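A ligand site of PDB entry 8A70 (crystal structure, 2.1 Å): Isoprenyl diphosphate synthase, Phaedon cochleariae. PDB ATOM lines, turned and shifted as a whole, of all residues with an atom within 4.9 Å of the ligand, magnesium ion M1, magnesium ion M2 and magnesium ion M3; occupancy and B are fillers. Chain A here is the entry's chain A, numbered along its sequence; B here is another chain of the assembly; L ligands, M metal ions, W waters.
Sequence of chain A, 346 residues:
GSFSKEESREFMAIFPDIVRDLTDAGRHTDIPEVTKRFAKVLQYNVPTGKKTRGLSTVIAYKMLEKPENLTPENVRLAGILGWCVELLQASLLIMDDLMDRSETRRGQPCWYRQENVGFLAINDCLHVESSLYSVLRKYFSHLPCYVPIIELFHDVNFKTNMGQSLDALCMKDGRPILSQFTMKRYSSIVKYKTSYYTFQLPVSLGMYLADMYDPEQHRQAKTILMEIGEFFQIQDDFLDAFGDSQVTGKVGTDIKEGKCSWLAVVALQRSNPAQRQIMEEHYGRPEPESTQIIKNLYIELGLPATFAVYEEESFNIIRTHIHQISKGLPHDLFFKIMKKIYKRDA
Water W9 binds magnesium ion M2. Magnesium ion M2 is bound by water W5 (2.1 Å). Magnesium ion M2 is bound by an oxygen (O2) of the ligand (2.1 Å). Water W12 binds magnesium ion M2 (2.2 Å). The side-chain carboxylate (OD2) of Asp 96 binds magnesium ion M2, at 2.3 Å. Magnesium ion M2 is bound by OD1 of Asp 100, 2.4 Å away. Magnesium ion M2 has six donor atoms within binding distance.
Merely in contact with magnesium ion M1: Arg 105 (3.8 Å). Three residues have an atom within 4 Å of magnesium ion M1: Asp 96, Asp 100 and Arg 105.
Asp 167 touches magnesium ion M2 (OD2 to MG, 3.9 Å). Within 4 Å of magnesium ion M2: Asp 96, Asp 100 and Asp 167.
The guanidinium group (NH2) of Arg 105 lies close to the side-chain carboxylate (OD1) of Asp 96. The side-chain carboxylate (OD2) of Asp 96 sits close to the side-chain amide nitrogen (NE2) of Gln 164 (3.2 Å). The guanidinium group (NH2) of Arg 105 is in salt-bridge range of the side-chain carboxylate (OD1) of Asp 97 (2.8 Å). The side-chain sulfur (SD) of Met 99 lies within hydrogen-bond range of the side-chain amide nitrogen (NE2) of Gln 164 (3.2 Å). O of Asn 123 of chain B lies close to OD1 of Asn 161, at 3.1 Å.
Residues that only touch magnesium ion M3: Lys 259 (3.9 Å). Of the 21 residues printed, 1 comes within 4 Å of magnesium ion M3.
Water W2 lies within hydrogen-bond range of OG of Ser 102 (2.6 Å), OD1 of Asp 97 (2.9 Å) and NH2 of Arg 105 (3.3 Å). Water W9 lies within hydrogen-bond range of OD2 of Asp 100 (2.5 Å) and NE2 of Gln 164 (3.1 Å). Water W12 bridges OD2 of Asp 167 and O3 of the ligand. Water W4 bridges the side-chain hydroxyl (OG) of Ser 102 (3.0 Å) and the side-chain carboxylate (OE1) of Glu 257 (3.0 Å). Water W10 bridges O3 of the ligand (2.9 Å) and NZ of Lys 259 (3.2 Å). Water W3 bridges the side-chain amino group (NZ) of Lys 193 and an oxygen (O1) of the ligand.
Magnesium ion M1 is bound by O5 of the ligand (1.9 Å), water W11 (2.0 Å), OD1 of Asp 100 (2.1 Å), O2 of the ligand (2.2 Å), OD1 of Asp 96 (2.2 Å) and water W2 (2.3 Å). Magnesium ion M1 has six donor atoms within binding distance.
Merely in contact with the ligand: Leu 92 (3.5 Å), Leu 93 (3.96 Å), Met 95 (3.9 Å), Thr 160 (3.9 Å), Asn 161 (3.5 Å), Gln 164 (3.4 Å) and Tyr 197 (3.4 Å). Hydrophobic or aromatic side chains within 4 Å of the ligand: Leu 92, Leu 93, Met 95 and Tyr 197.
NZ of Lys 259 lies within salt-bridge range of O3 of the ligand, 3.8 Å away. NH1 of Arg 105 lies within salt-bridge range of O6 of the ligand (2.9 Å). O3 of the ligand is in salt-bridge range of NZ of Lys 193 (3.5 Å).
Magnesium ion M3 is bound by O7 of the ligand, at 2.1 Å. Water W14 binds magnesium ion M3, at 2.2 Å. Magnesium ion M3 is bound by water W6 (2.2 Å). Magnesium ion M3 is bound by water W8 (2.2 Å). Water W4 is bound to magnesium ion M3 (2.2 Å). Magnesium ion M3 is bound by water W1 (2.3 Å).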
ATOM      1  N   LEU A  92      -5.564  33.670 -10.712  1.00  0.00           N
ATOM      2  CA  LEU A  92      -6.793  32.824 -10.657  1.00  0.00           C
ATOM      3  C   LEU A  92      -6.824  31.872 -11.867  1.00  0.00           C
ATOM      4  O   LEU A  92      -7.142  30.687 -11.670  1.00  0.00           O
ATOM      5  CB  LEU A  92      -8.041  33.712 -10.625  1.00  0.00           C
ATOM      6  CG  LEU A  92      -8.185  34.614  -9.403  1.00  0.00           C
ATOM      7  CD1 LEU A  92      -9.318  35.607  -9.603  1.00  0.00           C
ATOM      8  CD2 LEU A  92      -8.392  33.803  -8.142  1.00  0.00           C
ATOM      9  N   LEU A  93      -6.512  32.387 -13.062  1.00  0.00           N
ATOM     10  CA  LEU A  93      -6.640  31.649 -14.343  1.00  0.00           C
ATOM     11  C   LEU A  93      -5.488  30.635 -14.499  1.00  0.00           C
ATOM     12  O   LEU A  93      -5.755  29.549 -15.055  1.00  0.00           O
ATOM     13  CB  LEU A  93      -6.688  32.652 -15.509  1.00  0.00           C
ATOM     14  CG  LEU A  93      -7.875  33.606 -15.505  1.00  0.00           C
ATOM     15  CD1 LEU A  93      -7.883  34.468 -16.750  1.00  0.00           C
ATOM     16  CD2 LEU A  93      -9.199  32.847 -15.382  1.00  0.00           C
ATOM     17  N   MET A  95      -4.208  28.995 -11.980  1.00  0.00           N
ATOM     18  CA  MET A  95      -4.631  27.915 -11.056  1.00  0.00           C
ATOM     19  C   MET A  95      -5.810  27.150 -11.665  1.00  0.00           C
ATOM     20  O   MET A  95      -5.772  25.905 -11.648  1.00  0.00           O
ATOM     21  CB  MET A  95      -5.051  28.463  -9.686  1.00  0.00           C
ATOM     22  CG  MET A  95      -5.596  27.403  -8.755  1.00  0.00           C
ATOM     23  SD  MET A  95      -5.481  27.867  -7.021  1.00  0.00           S
ATOM     24  CE  MET A  95      -3.754  27.539  -6.703  1.00  0.00           C
ATOM     25  N   ASP A  96      -6.813  27.860 -12.166  1.00  0.00           N
ATOM     26  CA  ASP A  96      -8.057  27.264 -12.726  1.00  0.00           C
ATOM     27  C   ASP A  96      -7.694  26.328 -13.885  1.00  0.00           C
ATOM     28  O   ASP A  96      -8.279  25.224 -13.942  1.00  0.00           O
ATOM     29  CB  ASP A  96      -9.046  28.345 -13.196  1.00  0.00           C
ATOM     30  CG  ASP A  96     -10.284  27.741 -13.832  1.00  0.00           C
ATOM     31  OD1 ASP A  96     -10.354  27.733 -15.070  1.00  0.00           O
ATOM     32  OD2 ASP A  96     -11.163  27.268 -13.074  1.00  0.00           O
ATOM     33  N   ASP A  97      -6.775  26.734 -14.753  1.00  0.00           N
ATOM     34  CA  ASP A  97      -6.328  25.950 -15.936  1.00  0.00           C
ATOM     35  C   ASP A  97      -5.736  24.621 -15.452  1.00  0.00           C
ATOM     36  O   ASP A  97      -6.082  23.586 -16.058  1.00  0.00           O
ATOM     37  CB  ASP A  97      -5.350  26.754 -16.811  1.00  0.00           C
ATOM     38  CG  ASP A  97      -6.036  27.766 -17.712  1.00  0.00           C
ATOM     39  OD1 ASP A  97      -7.235  27.567 -18.025  1.00  0.00           O
ATOM     40  OD2 ASP A  97      -5.377  28.739 -18.113  1.00  0.00           O
ATOM     41  N   MET A  99      -6.401  23.159 -12.509  1.00  0.00           N
ATOM     42  CA  MET A  99      -7.556  22.458 -11.868  1.00  0.00           C
ATOM     43  C   MET A  99      -8.435  21.801 -12.935  1.00  0.00           C
ATOM     44  O   MET A  99      -8.825  20.631 -12.737  1.00  0.00           O
ATOM     45  CB  MET A  99      -8.389  23.440 -11.038  1.00  0.00           C
ATOM     46  CG  MET A  99      -7.753  23.779  -9.700  1.00  0.00           C
ATOM     47  SD  MET A  99      -8.696  24.961  -8.701  1.00  0.00           S
ATOM     48  CE  MET A  99     -10.153  23.994  -8.325  1.00  0.00           C
ATOM     49  N   ASP A 100      -8.720  22.509 -14.033  1.00  0.00           N
ATOM     50  CA  ASP A 100      -9.640  22.045 -15.120  1.00  0.00           C
ATOM     51  C   ASP A 100      -8.868  21.223 -16.168  1.00  0.00           C
ATOM     52  O   ASP A 100      -9.522  20.655 -17.061  1.00  0.00           O
ATOM     53  CB  ASP A 100     -10.348  23.226 -15.765  1.00  0.00           C
ATOM     54  CG  ASP A 100     -11.277  23.958 -14.804  1.00  0.00           C
ATOM     55  OD1 ASP A 100     -11.735  25.048 -15.165  1.00  0.00           O
ATOM     56  OD2 ASP A 100     -11.513  23.418 -13.708  1.00  0.00           O
ATOM     57  N   SER A 102      -7.161  22.281 -18.602  1.00  0.00           N
ATOM     58  CA  SER A 102      -7.454  22.929 -19.908  1.00  0.00           C
ATOM     59  C   SER A 102      -6.174  22.969 -20.756  1.00  0.00           C
ATOM     60  O   SER A 102      -5.066  22.954 -20.164  1.00  0.00           O
ATOM     61  CB  SER A 102      -8.038  24.307 -19.725  1.00  0.00           C
ATOM     62  OG  SER A 102      -9.345  24.229 -19.190  1.00  0.00           O
ATOM     63  N   ARG A 105      -5.911  28.946 -23.195  1.00  0.00           N
ATOM     64  CA  ARG A 105      -6.746  30.101 -22.742  1.00  0.00           C
ATOM     65  C   ARG A 105      -6.476  31.272 -23.696  1.00  0.00           C
ATOM     66  O   ARG A 105      -5.328  31.753 -23.720  1.00  0.00           O
ATOM     67  CB  ARG A 105      -6.429  30.484 -21.295  1.00  0.00           C
ATOM     68  CG  ARG A 105      -7.288  31.625 -20.770  1.00  0.00           C
ATOM     69  CD  ARG A 105      -7.173  31.842 -19.282  1.00  0.00           C
ATOM     70  NE  ARG A 105      -7.682  30.717 -18.501  1.00  0.00           N
ATOM     71  CZ  ARG A 105      -8.970  30.478 -18.250  1.00  0.00           C
ATOM     72  NH1 ARG A 105      -9.919  31.268 -18.721  1.00  0.00           N
ATOM     73  NH2 ARG A 105      -9.298  29.426 -17.516  1.00  0.00           N
ATOM     74  N   THR A 160     -13.649  34.880  -3.947  1.00  0.00           N
ATOM     75  CA  THR A 160     -13.433  34.200  -5.254  1.00  0.00           C
ATOM     76  C   THR A 160     -13.123  32.722  -4.999  1.00  0.00           C
ATOM     77  O   THR A 160     -13.630  31.875  -5.773  1.00  0.00           O
ATOM     78  CB  THR A 160     -12.340  34.902  -6.077  1.00  0.00           C
ATOM     79  OG1 THR A 160     -12.714  36.273  -6.243  1.00  0.00           O
ATOM     80  CG2 THR A 160     -12.142  34.271  -7.441  1.00  0.00           C
ATOM     81  N   ASN A 161     -12.349  32.420  -3.959  1.00  0.00           N
ATOM     82  CA  ASN A 161     -11.988  31.035  -3.554  1.00  0.00           C
ATOM     83  C   ASN A 161     -13.240  30.264  -3.116  1.00  0.00           C
ATOM     84  O   ASN A 161     -13.329  29.065  -3.440  1.00  0.00           O
ATOM     85  CB  ASN A 161     -10.901  31.033  -2.482  1.00  0.00           C
ATOM     86  CG  ASN A 161      -9.515  30.992  -3.083  1.00  0.00           C
ATOM     87  OD1 ASN A 161      -9.089  29.958  -3.595  1.00  0.00           O
ATOM     88  ND2 ASN A 161      -8.811  32.108  -3.034  1.00  0.00           N
ATOM     89  N   GLN A 164     -15.013  29.375  -6.378  1.00  0.00           N
ATOM     90  CA  GLN A 164     -14.310  28.267  -7.078  1.00  0.00           C
ATOM     91  C   GLN A 164     -14.642  26.933  -6.389  1.00  0.00           C
ATOM     92  O   GLN A 164     -14.909  25.950  -7.102  1.00  0.00           O
ATOM     93  CB  GLN A 164     -12.809  28.530  -7.120  1.00  0.00           C
ATOM     94  CG  GLN A 164     -11.982  27.419  -7.780  1.00  0.00           C
ATOM     95  CD  GLN A 164     -12.050  27.423  -9.288  1.00  0.00           C
ATOM     96  OE1 GLN A 164     -12.982  27.971  -9.888  1.00  0.00           O
ATOM     97  NE2 GLN A 164     -11.062  26.813  -9.922  1.00  0.00           N
ATOM     98  N   ASP A 167     -18.265  25.885  -7.069  1.00  0.00           N
ATOM     99  CA  ASP A 167     -18.261  25.360  -8.454  1.00  0.00           C
ATOM    100  C   ASP A 167     -17.817  23.890  -8.453  1.00  0.00           C
ATOM    101  O   ASP A 167     -18.455  23.084  -9.158  1.00  0.00           O
ATOM    102  CB  ASP A 167     -17.338  26.199  -9.355  1.00  0.00           C
ATOM    103  CG  ASP A 167     -17.568  26.015 -10.843  1.00  0.00           C
ATOM    104  OD1 ASP A 167     -18.733  25.826 -11.241  1.00  0.00           O
ATOM    105  OD2 ASP A 167     -16.575  26.075 -11.594  1.00  0.00           O
ATOM    106  N   LYS A 193     -17.510  33.661  -7.604  1.00  0.00           N
ATOM    107  CA  LYS A 193     -16.383  33.221  -8.472  1.00  0.00           C
ATOM    108  C   LYS A 193     -16.017  34.306  -9.494  1.00  0.00           C
ATOM    109  O   LYS A 193     -14.828  34.378  -9.840  1.00  0.00           O
ATOM    110  CB  LYS A 193     -16.687  31.909  -9.189  1.00  0.00           C
ATOM    111  CG  LYS A 193     -15.472  31.246  -9.831  1.00  0.00           C
ATOM    112  CD  LYS A 193     -15.736  29.858 -10.366  1.00  0.00           C
ATOM    113  CE  LYS A 193     -16.676  29.816 -11.561  1.00  0.00           C
ATOM    114  NZ  LYS A 193     -16.097  30.486 -12.744  1.00  0.00           N
ATOM    115  N   TYR A 197     -14.711  40.022  -8.391  1.00  0.00           N
ATOM    116  CA  TYR A 197     -13.385  40.394  -8.950  1.00  0.00           C
ATOM    117  C   TYR A 197     -13.567  41.101 -10.311  1.00  0.00           C
ATOM    118  O   TYR A 197     -12.696  41.915 -10.657  1.00  0.00           O
ATOM    119  CB  TYR A 197     -12.439  39.185  -9.011  1.00  0.00           C
ATOM    120  CG  TYR A 197     -12.350  38.467 -10.328  1.00  0.00           C
ATOM    121  CD1 TYR A 197     -11.549  38.945 -11.351  1.00  0.00           C
ATOM    122  CD2 TYR A 197     -13.028  37.281 -10.549  1.00  0.00           C
ATOM    123  CE1 TYR A 197     -11.439  38.281 -12.569  1.00  0.00           C
ATOM    124  CE2 TYR A 197     -12.935  36.600 -11.750  1.00  0.00           C
ATOM    125  CZ  TYR A 197     -12.136  37.097 -12.766  1.00  0.00           C
ATOM    126  OH  TYR A 197     -12.044  36.431 -13.952  1.00  0.00           O
ATOM    127  N   LYS A 250     -13.560  32.036 -30.091  1.00  0.00           N
ATOM    128  CA  LYS A 250     -13.192  30.815 -29.309  1.00  0.00           C
ATOM    129  C   LYS A 250     -14.205  29.708 -29.599  1.00  0.00           C
ATOM    130  O   LYS A 250     -15.366  30.029 -29.911  1.00  0.00           O
ATOM    131  CB  LYS A 250     -13.128  31.141 -27.814  1.00  0.00           C
ATOM    132  CG  LYS A 250     -12.279  30.183 -26.975  1.00  0.00           C
ATOM    133  CD  LYS A 250     -11.970  30.708 -25.578  1.00  0.00           C
ATOM    134  CE  LYS A 250     -10.894  29.906 -24.871  1.00  0.00           C
ATOM    135  NZ  LYS A 250     -10.683  30.386 -23.489  1.00  0.00           N
ATOM    136  N   THR A 253     -16.430  24.787 -25.008  1.00  0.00           N
ATOM    137  CA  THR A 253     -16.183  23.426 -24.447  1.00  0.00           C
ATOM    138  C   THR A 253     -16.852  23.258 -23.077  1.00  0.00           C
ATOM    139  O   THR A 253     -16.458  22.331 -22.353  1.00  0.00           O
ATOM    140  CB  THR A 253     -14.679  23.154 -24.363  1.00  0.00           C
ATOM    141  OG1 THR A 253     -14.077  24.226 -23.644  1.00  0.00           O
ATOM    142  CG2 THR A 253     -14.018  23.022 -25.721  1.00  0.00           C
ATOM    143  N   GLU A 257     -16.711  19.800 -20.669  1.00  0.00           N
ATOM    144  CA  GLU A 257     -16.073  20.015 -19.337  1.00  0.00           C
ATOM    145  C   GLU A 257     -17.092  19.763 -18.223  1.00  0.00           C
ATOM    146  O   GLU A 257     -16.664  19.675 -17.050  1.00  0.00           O
ATOM    147  CB  GLU A 257     -15.498  21.427 -19.257  1.00  0.00           C
ATOM    148  CG  GLU A 257     -14.286  21.616 -20.158  1.00  0.00           C
ATOM    149  CD  GLU A 257     -13.694  23.016 -20.135  1.00  0.00           C
ATOM    150  OE1 GLU A 257     -12.888  23.298 -19.231  1.00  0.00           O
ATOM    151  OE2 GLU A 257     -14.066  23.826 -21.014  1.00  0.00           O
ATOM    152  N   LYS A 259     -19.591  21.749 -17.105  1.00  0.00           N
ATOM    153  CA  LYS A 259     -19.725  22.981 -16.286  1.00  0.00           C
ATOM    154  C   LYS A 259     -21.185  23.153 -15.848  1.00  0.00           C
ATOM    155  O   LYS A 259     -22.092  22.767 -16.617  1.00  0.00           O
ATOM    156  CB  LYS A 259     -19.301  24.228 -17.074  1.00  0.00           C
ATOM    157  CG  LYS A 259     -17.809  24.322 -17.379  1.00  0.00           C
ATOM    158  CD  LYS A 259     -17.370  25.731 -17.686  1.00  0.00           C
ATOM    159  CE  LYS A 259     -15.938  25.804 -18.171  1.00  0.00           C
ATOM    160  NZ  LYS A 259     -15.683  27.055 -18.920  1.00  0.00           N
ATOM    161  N   ASN B 123      -7.071  24.855  -4.967  1.00  0.00           N
ATOM    162  CA  ASN B 123      -7.291  26.274  -4.555  1.00  0.00           C
ATOM    163  C   ASN B 123      -7.457  26.395  -3.038  1.00  0.00           C
ATOM    164  O   ASN B 123      -7.533  27.541  -2.556  1.00  0.00           O
ATOM    165  CB  ASN B 123      -8.481  26.896  -5.286  1.00  0.00           C
ATOM    166  CG  ASN B 123      -9.818  26.403  -4.783  1.00  0.00           C
ATOM    167  OD1 ASN B 123     -10.115  25.211  -4.886  1.00  0.00           O
ATOM    168  ND2 ASN B 123     -10.632  27.304  -4.254  1.00  0.00           N
ATOM    169  N   LEU B 126      -4.521  28.369  -1.707  1.00  0.00           N
ATOM    170  CA  LEU B 126      -4.717  29.828  -1.936  1.00  0.00           C
ATOM    171  C   LEU B 126      -5.735  30.379  -0.928  1.00  0.00           C
ATOM    172  O   LEU B 126      -5.502  31.481  -0.395  1.00  0.00           O
ATOM    173  CB  LEU B 126      -5.179  30.074  -3.382  1.00  0.00           C
ATOM    174  CG  LEU B 126      -5.365  31.542  -3.768  1.00  0.00           C
ATOM    175  CD1 LEU B 126      -4.060  32.311  -3.696  1.00  0.00           C
ATOM    176  CD2 LEU B 126      -5.973  31.666  -5.164  1.00  0.00           C
HETATM  177  C1  LIG L   1     -12.663  30.311 -14.733  1.00  0.00           C
HETATM  178  O1  LIG L   1     -13.969  29.724 -14.684  1.00  0.00           O
HETATM  179  C2  LIG L   1     -12.180  30.612 -13.349  1.00  0.00           C
HETATM  180  C3  LIG L   1     -12.220  31.785 -12.715  1.00  0.00           C
HETATM  181  C4  LIG L   1     -12.608  33.076 -13.389  1.00  0.00           C
HETATM  182  C5  LIG L   1     -11.897  31.922 -11.252  1.00  0.00           C
HETATM  183  C6  LIG L   1     -11.067  30.813 -10.638  1.00  0.00           C
HETATM  184  C7  LIG L   1     -10.878  30.987  -9.160  1.00  0.00           C
HETATM  185  C8  LIG L   1     -10.008  30.387  -8.349  1.00  0.00           C
HETATM  186  C9  LIG L   1      -8.910  29.487  -8.843  1.00  0.00           C
HETATM  187  C10 LIG L   1     -10.058  30.539  -6.865  1.00  0.00           C
HETATM  188  P1  LIG L   1     -14.272  28.351 -15.473  1.00  0.00           P
HETATM  189  O2  LIG L   1     -13.211  27.346 -15.155  1.00  0.00           O
HETATM  190  O3  LIG L   1     -15.687  27.979 -15.200  1.00  0.00           O
HETATM  191  O4  LIG L   1     -14.137  28.812 -17.005  1.00  0.00           O
HETATM  192  P2  LIG L   1     -12.934  28.962 -18.086  1.00  0.00           P
HETATM  193  O5  LIG L   1     -11.744  28.228 -17.526  1.00  0.00           O
HETATM  194  O6  LIG L   1     -12.693  30.442 -18.235  1.00  0.00           O
HETATM  195  O7  LIG L   1     -13.455  28.328 -19.359  1.00  0.00           O
HETATM  196 MG    MG M   1     -11.676  26.653 -16.510  1.00  0.00          MG
HETATM  197 MG    MG M   2     -13.119  26.075 -13.436  1.00  0.00          MG
HETATM  198 MG    MG M   3     -12.522  27.657 -21.102  1.00  0.00          MG
HETATM  199  O   HOH W   1     -10.882  29.204 -20.841  1.00  0.00           O
HETATM  200  O   HOH W   2      -9.666  26.180 -17.475  1.00  0.00           O
HETATM  201  O   HOH W   3     -16.702  31.640 -15.249  1.00  0.00           O
HETATM  202  O   HOH W   4     -11.587  25.743 -20.445  1.00  0.00           O
HETATM  203  O   HOH W   5     -14.156  27.438 -12.203  1.00  0.00           O
HETATM  204  O   HOH W   6     -13.696  29.299 -21.989  1.00  0.00           O
HETATM  205  O   HOH W   7     -13.253  31.628 -20.630  1.00  0.00           O
HETATM  206  O   HOH W   8     -12.254  27.202 -23.259  1.00  0.00           O
HETATM  207  O   HOH W   9     -12.441  24.916 -11.981  1.00  0.00           O
HETATM  208  O   HOH W  10     -17.602  28.978 -17.194  1.00  0.00           O
HETATM  209  O   HOH W  11     -12.567  25.310 -17.770  1.00  0.00           O
HETATM  210  O   HOH W  12     -14.890  24.934 -13.978  1.00  0.00           O
HETATM  211  O   HOH W  13     -14.455  35.333 -15.281  1.00  0.00           O
HETATM  212  O   HOH W  14     -14.397  26.615 -21.519  1.00  0.00           O
